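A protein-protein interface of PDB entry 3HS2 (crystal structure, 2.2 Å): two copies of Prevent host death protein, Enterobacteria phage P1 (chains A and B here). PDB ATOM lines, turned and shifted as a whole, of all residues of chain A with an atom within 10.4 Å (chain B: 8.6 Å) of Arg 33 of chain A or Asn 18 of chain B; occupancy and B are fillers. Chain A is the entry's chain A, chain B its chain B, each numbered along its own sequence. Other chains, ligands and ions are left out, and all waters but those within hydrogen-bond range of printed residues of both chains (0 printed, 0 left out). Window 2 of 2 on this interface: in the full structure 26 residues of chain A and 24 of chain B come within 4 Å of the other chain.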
ATOM      1  N   ILE A   4       7.227  -2.450 -19.049  1.00  0.00           N
ATOM      2  CA  ILE A   4       6.902  -1.430 -18.067  1.00  0.00           C
ATOM      3  C   ILE A   4       5.394  -1.282 -17.926  1.00  0.00           C
ATOM      4  O   ILE A   4       4.639  -1.601 -18.846  1.00  0.00           O
ATOM      5  CB  ILE A   4       7.490  -0.073 -18.465  1.00  0.00           C
ATOM      6  CG1 ILE A   4       6.982   0.322 -19.853  1.00  0.00           C
ATOM      7  CG2 ILE A   4       9.013  -0.124 -18.443  1.00  0.00           C
ATOM      8  CD1 ILE A   4       7.321   1.733 -20.255  1.00  0.00           C
ATOM      9  N   ASN A   5       4.959  -0.798 -16.768  1.00  0.00           N
ATOM     10  CA  ASN A   5       3.538  -0.572 -16.538  1.00  0.00           C
ATOM     11  C   ASN A   5       3.078   0.787 -17.055  1.00  0.00           C
ATOM     12  O   ASN A   5       3.894   1.635 -17.412  1.00  0.00           O
ATOM     13  CB  ASN A   5       3.179  -0.745 -15.058  1.00  0.00           C
ATOM     14  CG  ASN A   5       3.888   0.248 -14.164  1.00  0.00           C
ATOM     15  OD1 ASN A   5       3.991   1.427 -14.485  1.00  0.00           O
ATOM     16  ND2 ASN A   5       4.377  -0.227 -13.030  1.00  0.00           N
ATOM     17  N   PHE A   6       1.767   0.983 -17.088  1.00  0.00           N
ATOM     18  CA  PHE A   6       1.179   2.188 -17.647  1.00  0.00           C
ATOM     19  C   PHE A   6       1.681   3.463 -16.975  1.00  0.00           C
ATOM     20  O   PHE A   6       2.137   4.384 -17.650  1.00  0.00           O
ATOM     21  CB  PHE A   6      -0.341   2.127 -17.562  1.00  0.00           C
ATOM     22  CG  PHE A   6      -1.016   3.361 -18.066  1.00  0.00           C
ATOM     23  CD1 PHE A   6      -1.161   3.575 -19.423  1.00  0.00           C
ATOM     24  CD2 PHE A   6      -1.500   4.312 -17.188  1.00  0.00           C
ATOM     25  CE1 PHE A   6      -1.779   4.708 -19.896  1.00  0.00           C
ATOM     26  CE2 PHE A   6      -2.121   5.449 -17.657  1.00  0.00           C
ATOM     27  CZ  PHE A   6      -2.262   5.646 -19.013  1.00  0.00           C
ATOM     28  N   GLU A  27       7.532  -3.119 -24.004  1.00  0.00           N
ATOM     29  CA  GLU A  27       6.191  -3.594 -23.722  1.00  0.00           C
ATOM     30  C   GLU A  27       5.548  -2.728 -22.652  1.00  0.00           C
ATOM     31  O   GLU A  27       6.145  -2.451 -21.613  1.00  0.00           O
ATOM     32  CB  GLU A  27       6.232  -5.054 -23.267  1.00  0.00           C
ATOM     33  CG  GLU A  27       4.879  -5.641 -22.897  1.00  0.00           C
ATOM     34  CD  GLU A  27       4.995  -7.033 -22.306  1.00  0.00           C
ATOM     35  OE1 GLU A  27       6.118  -7.580 -22.292  1.00  0.00           O
ATOM     36  OE2 GLU A  27       3.969  -7.583 -21.855  1.00  0.00           O
ATOM     37  N   ILE A  28       4.331  -2.285 -22.925  1.00  0.00           N
ATOM     38  CA  ILE A  28       3.558  -1.544 -21.952  1.00  0.00           C
ATOM     39  C   ILE A  28       2.444  -2.447 -21.447  1.00  0.00           C
ATOM     40  O   ILE A  28       1.649  -2.957 -22.230  1.00  0.00           O
ATOM     41  CB  ILE A  28       2.954  -0.275 -22.569  1.00  0.00           C
ATOM     42  CG1 ILE A  28       4.061   0.618 -23.131  1.00  0.00           C
ATOM     43  CG2 ILE A  28       2.124   0.472 -21.541  1.00  0.00           C
ATOM     44  CD1 ILE A  28       3.550   1.856 -23.820  1.00  0.00           C
ATOM     45  N   THR A  29       2.403  -2.661 -20.138  1.00  0.00           N
ATOM     46  CA  THR A  29       1.374  -3.497 -19.545  1.00  0.00           C
ATOM     47  C   THR A  29       0.333  -2.632 -18.855  1.00  0.00           C
ATOM     48  O   THR A  29       0.625  -1.517 -18.426  1.00  0.00           O
ATOM     49  CB  THR A  29       1.969  -4.491 -18.527  1.00  0.00           C
ATOM     50  OG1 THR A  29       2.619  -3.771 -17.471  1.00  0.00           O
ATOM     51  CG2 THR A  29       2.981  -5.402 -19.204  1.00  0.00           C
ATOM     52  N   ARG A  30      -0.886  -3.150 -18.765  1.00  0.00           N
ATOM     53  CA  ARG A  30      -1.969  -2.460 -18.081  1.00  0.00           C
ATOM     54  C   ARG A  30      -2.788  -3.453 -17.270  1.00  0.00           C
ATOM     55  O   ARG A  30      -3.009  -4.582 -17.704  1.00  0.00           O
ATOM     56  CB  ARG A  30      -2.866  -1.737 -19.084  1.00  0.00           C
ATOM     57  CG  ARG A  30      -2.289  -0.435 -19.597  1.00  0.00           C
ATOM     58  CD  ARG A  30      -3.380   0.461 -20.157  1.00  0.00           C
ATOM     59  NE  ARG A  30      -3.993  -0.102 -21.355  1.00  0.00           N
ATOM     60  CZ  ARG A  30      -5.101   0.371 -21.917  1.00  0.00           C
ATOM     61  NH1 ARG A  30      -5.729   1.413 -21.386  1.00  0.00           N
ATOM     62  NH2 ARG A  30      -5.586  -0.202 -23.007  1.00  0.00           N
ATOM     63  N   ARG A  31      -3.240  -3.035 -16.093  1.00  0.00           N
ATOM     64  CA  ARG A  31      -4.017  -3.924 -15.237  1.00  0.00           C
ATOM     65  C   ARG A  31      -5.374  -4.255 -15.851  1.00  0.00           C
ATOM     66  O   ARG A  31      -6.174  -3.364 -16.143  1.00  0.00           O
ATOM     67  CB  ARG A  31      -4.181  -3.337 -13.831  1.00  0.00           C
ATOM     68  CG  ARG A  31      -4.535  -1.858 -13.802  1.00  0.00           C
ATOM     69  N   GLY A  32      -5.621  -5.545 -16.050  1.00  0.00           N
ATOM     70  CA  GLY A  32      -6.874  -6.004 -16.625  1.00  0.00           C
ATOM     71  C   GLY A  32      -7.005  -5.716 -18.108  1.00  0.00           C
ATOM     72  O   GLY A  32      -8.108  -5.747 -18.655  1.00  0.00           O
ATOM     73  N   ARG A  33      -5.882  -5.438 -18.764  1.00  0.00           N
ATOM     74  CA  ARG A  33      -5.886  -5.106 -20.186  1.00  0.00           C
ATOM     75  C   ARG A  33      -4.800  -5.865 -20.942  1.00  0.00           C
ATOM     76  O   ARG A  33      -3.882  -6.411 -20.335  1.00  0.00           O
ATOM     77  CB  ARG A  33      -5.679  -3.603 -20.383  1.00  0.00           C
ATOM     78  CG  ARG A  33      -6.832  -2.740 -19.909  1.00  0.00           C
ATOM     79  CD  ARG A  33      -8.116  -3.104 -20.634  1.00  0.00           C
ATOM     80  NE  ARG A  33      -9.015  -1.963 -20.757  1.00  0.00           N
ATOM     81  CZ  ARG A  33      -9.144  -1.231 -21.858  1.00  0.00           C
ATOM     82  NH1 ARG A  33      -8.434  -1.523 -22.939  1.00  0.00           N
ATOM     83  NH2 ARG A  33      -9.987  -0.208 -21.881  1.00  0.00           N
ATOM     84  N   GLU A  34      -4.903  -5.884 -22.267  1.00  0.00           N
ATOM     85  CA  GLU A  34      -3.897  -6.528 -23.107  1.00  0.00           C
ATOM     86  C   GLU A  34      -2.676  -5.631 -23.276  1.00  0.00           C
ATOM     87  O   GLU A  34      -2.803  -4.413 -23.357  1.00  0.00           O
ATOM     88  CB  GLU A  34      -4.488  -6.879 -24.474  1.00  0.00           C
ATOM     89  CG  GLU A  34      -5.678  -7.820 -24.397  1.00  0.00           C
ATOM     90  CD  GLU A  34      -5.391  -9.050 -23.555  1.00  0.00           C
ATOM     91  OE1 GLU A  34      -6.252  -9.415 -22.726  1.00  0.00           O
ATOM     92  OE2 GLU A  34      -4.303  -9.646 -23.713  1.00  0.00           O
ATOM     93  N   PRO A  35      -1.478  -6.236 -23.323  1.00  0.00           N
ATOM     94  CA  PRO A  35      -0.255  -5.436 -23.419  1.00  0.00           C
ATOM     95  C   PRO A  35      -0.074  -4.822 -24.802  1.00  0.00           C
ATOM     96  O   PRO A  35      -0.532  -5.371 -25.806  1.00  0.00           O
ATOM     97  CB  PRO A  35       0.859  -6.457 -23.147  1.00  0.00           C
ATOM     98  CG  PRO A  35       0.171  -7.687 -22.633  1.00  0.00           C
ATOM     99  CD  PRO A  35      -1.188  -7.671 -23.245  1.00  0.00           C
ATOM    100  N   ALA A  36       0.591  -3.674 -24.835  1.00  0.00           N
ATOM    101  CA  ALA A  36       0.938  -3.023 -26.085  1.00  0.00           C
ATOM    102  C   ALA A  36       2.451  -3.018 -26.238  1.00  0.00           C
ATOM    103  O   ALA A  36       3.184  -3.181 -25.263  1.00  0.00           O
ATOM    104  CB  ALA A  36       0.398  -1.600 -26.109  1.00  0.00           C
ATOM    105  N   ASN B  12      -2.899  11.884 -23.626  1.00  0.00           N
ATOM    106  CA  ASN B  12      -4.020  11.002 -23.922  1.00  0.00           C
ATOM    107  C   ASN B  12      -3.612   9.534 -24.002  1.00  0.00           C
ATOM    108  O   ASN B  12      -4.237   8.754 -24.720  1.00  0.00           O
ATOM    109  CB  ASN B  12      -4.702  11.407 -25.234  1.00  0.00           C
ATOM    110  CG  ASN B  12      -5.102  12.867 -25.263  1.00  0.00           C
ATOM    111  OD1 ASN B  12      -4.268  13.746 -25.473  1.00  0.00           O
ATOM    112  ND2 ASN B  12      -6.387  13.133 -25.073  1.00  0.00           N
ATOM    113  N   LEU B  13      -2.578   9.152 -23.257  1.00  0.00           N
ATOM    114  CA  LEU B  13      -2.015   7.809 -23.382  1.00  0.00           C
ATOM    115  C   LEU B  13      -3.040   6.695 -23.180  1.00  0.00           C
ATOM    116  O   LEU B  13      -3.028   5.695 -23.896  1.00  0.00           O
ATOM    117  CB  LEU B  13      -0.819   7.622 -22.443  1.00  0.00           C
ATOM    118  CG  LEU B  13       0.045   6.391 -22.731  1.00  0.00           C
ATOM    119  CD1 LEU B  13       0.489   6.372 -24.185  1.00  0.00           C
ATOM    120  CD2 LEU B  13       1.246   6.318 -21.803  1.00  0.00           C
ATOM    121  N   SER B  14      -3.934   6.871 -22.213  1.00  0.00           N
ATOM    122  CA  SER B  14      -4.923   5.841 -21.913  1.00  0.00           C
ATOM    123  C   SER B  14      -5.820   5.521 -23.113  1.00  0.00           C
ATOM    124  O   SER B  14      -5.950   4.362 -23.506  1.00  0.00           O
ATOM    125  CB  SER B  14      -5.766   6.242 -20.702  1.00  0.00           C
ATOM    126  OG  SER B  14      -6.475   5.130 -20.200  1.00  0.00           O
ATOM    127  N   GLU B  15      -6.436   6.544 -23.696  1.00  0.00           N
ATOM    128  CA  GLU B  15      -7.323   6.335 -24.839  1.00  0.00           C
ATOM    129  C   GLU B  15      -6.564   5.831 -26.067  1.00  0.00           C
ATOM    130  O   GLU B  15      -7.098   5.061 -26.864  1.00  0.00           O
ATOM    131  CB  GLU B  15      -8.094   7.612 -25.171  1.00  0.00           C
ATOM    132  N   VAL B  16      -5.323   6.277 -26.214  1.00  0.00           N
ATOM    133  CA  VAL B  16      -4.452   5.789 -27.276  1.00  0.00           C
ATOM    134  C   VAL B  16      -4.273   4.273 -27.185  1.00  0.00           C
ATOM    135  O   VAL B  16      -4.358   3.570 -28.189  1.00  0.00           O
ATOM    136  CB  VAL B  16      -3.074   6.470 -27.207  1.00  0.00           C
ATOM    137  CG1 VAL B  16      -2.100   5.808 -28.166  1.00  0.00           C
ATOM    138  CG2 VAL B  16      -3.207   7.960 -27.498  1.00  0.00           C
ATOM    139  N   LEU B  17      -4.026   3.781 -25.975  1.00  0.00           N
ATOM    140  CA  LEU B  17      -3.856   2.354 -25.733  1.00  0.00           C
ATOM    141  C   LEU B  17      -5.165   1.597 -25.959  1.00  0.00           C
ATOM    142  O   LEU B  17      -5.163   0.461 -26.435  1.00  0.00           O
ATOM    143  CB  LEU B  17      -3.330   2.109 -24.315  1.00  0.00           C
ATOM    144  CG  LEU B  17      -1.889   2.541 -24.035  1.00  0.00           C
ATOM    145  CD1 LEU B  17      -1.480   2.207 -22.617  1.00  0.00           C
ATOM    146  CD2 LEU B  17      -0.961   1.873 -25.011  1.00  0.00           C
ATOM    147  N   ASN B  18      -6.280   2.230 -25.618  1.00  0.00           N
ATOM    148  CA  ASN B  18      -7.590   1.659 -25.896  1.00  0.00           C
ATOM    149  C   ASN B  18      -7.809   1.503 -27.398  1.00  0.00           C
ATOM    150  O   ASN B  18      -8.344   0.495 -27.853  1.00  0.00           O
ATOM    151  CB  ASN B  18      -8.694   2.512 -25.275  1.00  0.00           C
ATOM    152  CG  ASN B  18      -8.707   2.435 -23.753  1.00  0.00           C
ATOM    153  OD1 ASN B  18      -8.094   1.550 -23.157  1.00  0.00           O
ATOM    154  ND2 ASN B  18      -9.410   3.366 -23.124  1.00  0.00           N
ATOM    155  N   ASN B  19      -7.385   2.504 -28.163  1.00  0.00           N
ATOM    156  CA  ASN B  19      -7.431   2.428 -29.620  1.00  0.00           C
ATOM    157  C   ASN B  19      -6.560   1.298 -30.159  1.00  0.00           C
ATOM    158  O   ASN B  19      -6.967   0.560 -31.056  1.00  0.00           O
ATOM    159  CB  ASN B  19      -7.000   3.756 -30.242  1.00  0.00           C
ATOM    160  CG  ASN B  19      -8.067   4.832 -30.121  1.00  0.00           C
ATOM    161  OD1 ASN B  19      -9.240   4.539 -29.890  1.00  0.00           O
ATOM    162  ND2 ASN B  19      -7.662   6.086 -30.285  1.00  0.00           N
ATOM    163  N   VAL B  20      -5.355   1.170 -29.612  1.00  0.00           N
ATOM    164  CA  VAL B  20      -4.437   0.129 -30.055  1.00  0.00           C
ATOM    165  C   VAL B  20      -5.008  -1.254 -29.771  1.00  0.00           C
ATOM    166  O   VAL B  20      -4.966  -2.133 -30.628  1.00  0.00           O
ATOM    167  CB  VAL B  20      -3.056   0.267 -29.397  1.00  0.00           C
ATOM    168  CG1 VAL B  20      -2.212  -0.953 -29.692  1.00  0.00           C
ATOM    169  CG2 VAL B  20      -2.365   1.526 -29.890  1.00  0.00           C
ATOM    170  N   GLU B  21      -5.548  -1.443 -28.569  1.00  0.00           N
ATOM    171  CA  GLU B  21      -6.152  -2.719 -28.208  1.00  0.00           C
ATOM    172  C   GLU B  21      -7.343  -3.042 -29.102  1.00  0.00           C
ATOM    173  O   GLU B  21      -7.636  -4.207 -29.363  1.00  0.00           O
ATOM    174  CB  GLU B  21      -6.592  -2.727 -26.741  1.00  0.00           C
ATOM    175  CG  GLU B  21      -7.377  -3.975 -26.360  1.00  0.00           C
ATOM    176  CD  GLU B  21      -7.914  -3.943 -24.940  1.00  0.00           C
ATOM    177  OE1 GLU B  21      -9.150  -3.862 -24.773  1.00  0.00           O
ATOM    178  OE2 GLU B  21      -7.103  -4.009 -23.992  1.00  0.00           O
ATOM    179  N   ALA B  22      -8.026  -2.003 -29.572  1.00  0.00           N
ATOM    180  CA  ALA B  22      -9.200  -2.184 -30.412  1.00  0.00           C
ATOM    181  C   ALA B  22      -8.828  -2.726 -31.791  1.00  0.00           C
ATOM    182  O   ALA B  22      -9.691  -3.206 -32.529  1.00  0.00           O
ATOM    183  CB  ALA B  22      -9.971  -0.885 -30.534  1.00  0.00           C
ATOM    184  N   GLY B  23      -7.543  -2.642 -32.128  1.00  0.00           N
ATOM    185  CA  GLY B  23      -7.041  -3.175 -33.383  1.00  0.00           C
ATOM    186  C   GLY B  23      -6.301  -2.167 -34.246  1.00  0.00           C
ATOM    187  O   GLY B  23      -5.975  -2.457 -35.396  1.00  0.00           O
ATOM    188  N   GLU B  24      -6.028  -0.987 -33.697  1.00  0.00           N
ATOM    189  CA  GLU B  24      -5.374   0.079 -34.455  1.00  0.00           C
ATOM    190  C   GLU B  24      -3.871   0.175 -34.187  1.00  0.00           C
ATOM    191  O   GLU B  24      -3.397  -0.181 -33.109  1.00  0.00           O
ATOM    192  CB  GLU B  24      -6.034   1.425 -34.148  1.00  0.00           C
ATOM    193  N   VAL B  26      -0.820   2.989 -33.963  1.00  0.00           N
ATOM    194  CA  VAL B  26      -0.727   4.433 -33.782  1.00  0.00           C
ATOM    195  C   VAL B  26       0.700   4.949 -33.846  1.00  0.00           C
ATOM    196  O   VAL B  26       1.579   4.479 -33.126  1.00  0.00           O
ATOM    197  CB  VAL B  26      -1.374   4.886 -32.460  1.00  0.00           C
ATOM    198  CG1 VAL B  26      -1.416   6.401 -32.389  1.00  0.00           C
ATOM    199  CG2 VAL B  26      -2.769   4.314 -32.340  1.00  0.00           C
ATOM    200  N   ILE B  38       3.002   2.328 -31.888  1.00  0.00           N
ATOM    201  CA  ILE B  38       2.490   1.485 -30.819  1.00  0.00           C
ATOM    202  C   ILE B  38       1.385   0.569 -31.330  1.00  0.00           C
ATOM    203  O   ILE B  38       0.418   1.023 -31.942  1.00  0.00           O
ATOM    204  CB  ILE B  38       2.016   2.311 -29.612  1.00  0.00           C
ATOM    205  CG1 ILE B  38       1.003   1.513 -28.795  1.00  0.00           C
ATOM    206  CG2 ILE B  38       1.427   3.635 -30.064  1.00  0.00           C
ATOM    207  CD1 ILE B  38       1.063   1.820 -27.337  1.00  0.00           C
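The side-chain amide oxygen (OD1) of Asn 18 of chain B lies within hydrogen-bond range of the guanidinium group (NH1) of Arg 30 of chain A, at 3.0 Å.
NH2 of Arg 33 of chain A sits at hydrogen-bond distance from OD1 of Asn 18 of chain B.
The guanidinium group (NH1) of Arg 33 of chain A is in salt-bridge range of the side-chain carboxylate (OE2) of Glu 21 of chain B (3.0 Å).
N of Glu 34 of chain A lies within hydrogen-bond range of OE2 of Glu 21 of chain B, 3.4 Å away.
The backbone NH of Phe 6 of chain A is in hydrogen-bond range of the backbone carbonyl oxygen of Thr 29 of chain A (3.1 Å).
The backbone NH (N) of Ile 28 of chain A is in hydrogen-bond range of the backbone carbonyl oxygen (O) of Ala 36 of chain A, 2.8 Å away.
The backbone carbonyl oxygen of Val 26 of chain B lies within hydrogen-bond range of the backbone NH of Ile 38 of chain B, at 2.9 Å.
Among the printed residues, merely in contact across the chains: Phe 6 of chain A with Leu 13 of chain B (3.8 Å), Phe 6 of chain A with Ser 14 of chain B (3.8 Å), Phe 6 of chain A with Leu 17 of chain B (3.5 Å), Arg 30 of chain A with Ser 14 of chain B (3.6 Å), Arg 30 of chain A with Leu 17 of chain B (3.5 Å), Ala 36 of chain A with Leu 17 of chain B (3.9 Å) and Ala 36 of chain A with Ile 38 of chain B (3.7 Å).
Arg 33 of chain A touches just these residues of chain B: Asn 18 (2.9 Å) and Glu 21 (3.0 Å).
Printed residues of chain B within 4 Å of Glu 34 of chain A: Glu 21.
Printed residues of chain B within 4 Å of Ala 36 of chain A: Leu 17 and Ile 38.
Ser 14 of chain B touches two residues of chain A.
No residue of chain A comes within 4 Å of Glu 15 of chain B.
Of chain A, only Phe 6 (3.5 Å), Arg 30 (3.5 Å) and Ala 36 (3.9 Å) come within 4 Å of Leu 17 of chain B.
Asn 18 of chain B touches just these residues of chain A: Arg 30 and Arg 33.
No residue of chain A comes within 4 Å of Asn 19 of chain B.
Glu 21 of chain B touches just these residues of chain A: Arg 33 (3.0 Å) and Glu 34 (3.4 Å).
Gly 23 of chain B touches none of the printed residues of chain A.
Val 26 of chain B touches none of the printed residues of chain A.
Printed residues of chain A within 4 Å of Ile 38 of chain B: Ala 36.
The nearest residue of chain B that does not touch Arg 33 of chain A is Leu 17 of chain B (5.2 Å).
The nearest printed residue of chain A that does not touch Asn 18 of chain B is Phe 6 of chain A (7.7 Å).
The nearest printed residue of chain B that does not touch Glu 34 of chain A is Leu 17 of chain B (6.2 Å).
Hydrophobic or aromatic side chains of chain B within 4 Å of the printed part of chain A: Leu 13, Leu 17 and Ile 38.
Along chain B the printed residues that touch a printed residue of chain A span positions 13 to 38.
Of the 13 printed residues of chain A, 5 touch a printed residue of chain B.
Hydrophobic or aromatic side chains of chain A within 4 Å of the printed part of chain B: Phe 6 and Ala 36.
Among the printed residues, Asp or Glu carboxylates within 4 Å of a Lys or Arg side-chain nitrogen of the other chain: Arg 33 of chain A with Glu 21 of chain B.
No position is printed for both chains.
Of the 11 pairs that touch across the chains among the printed residues, none has its exchanged pair printed and touching as well.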
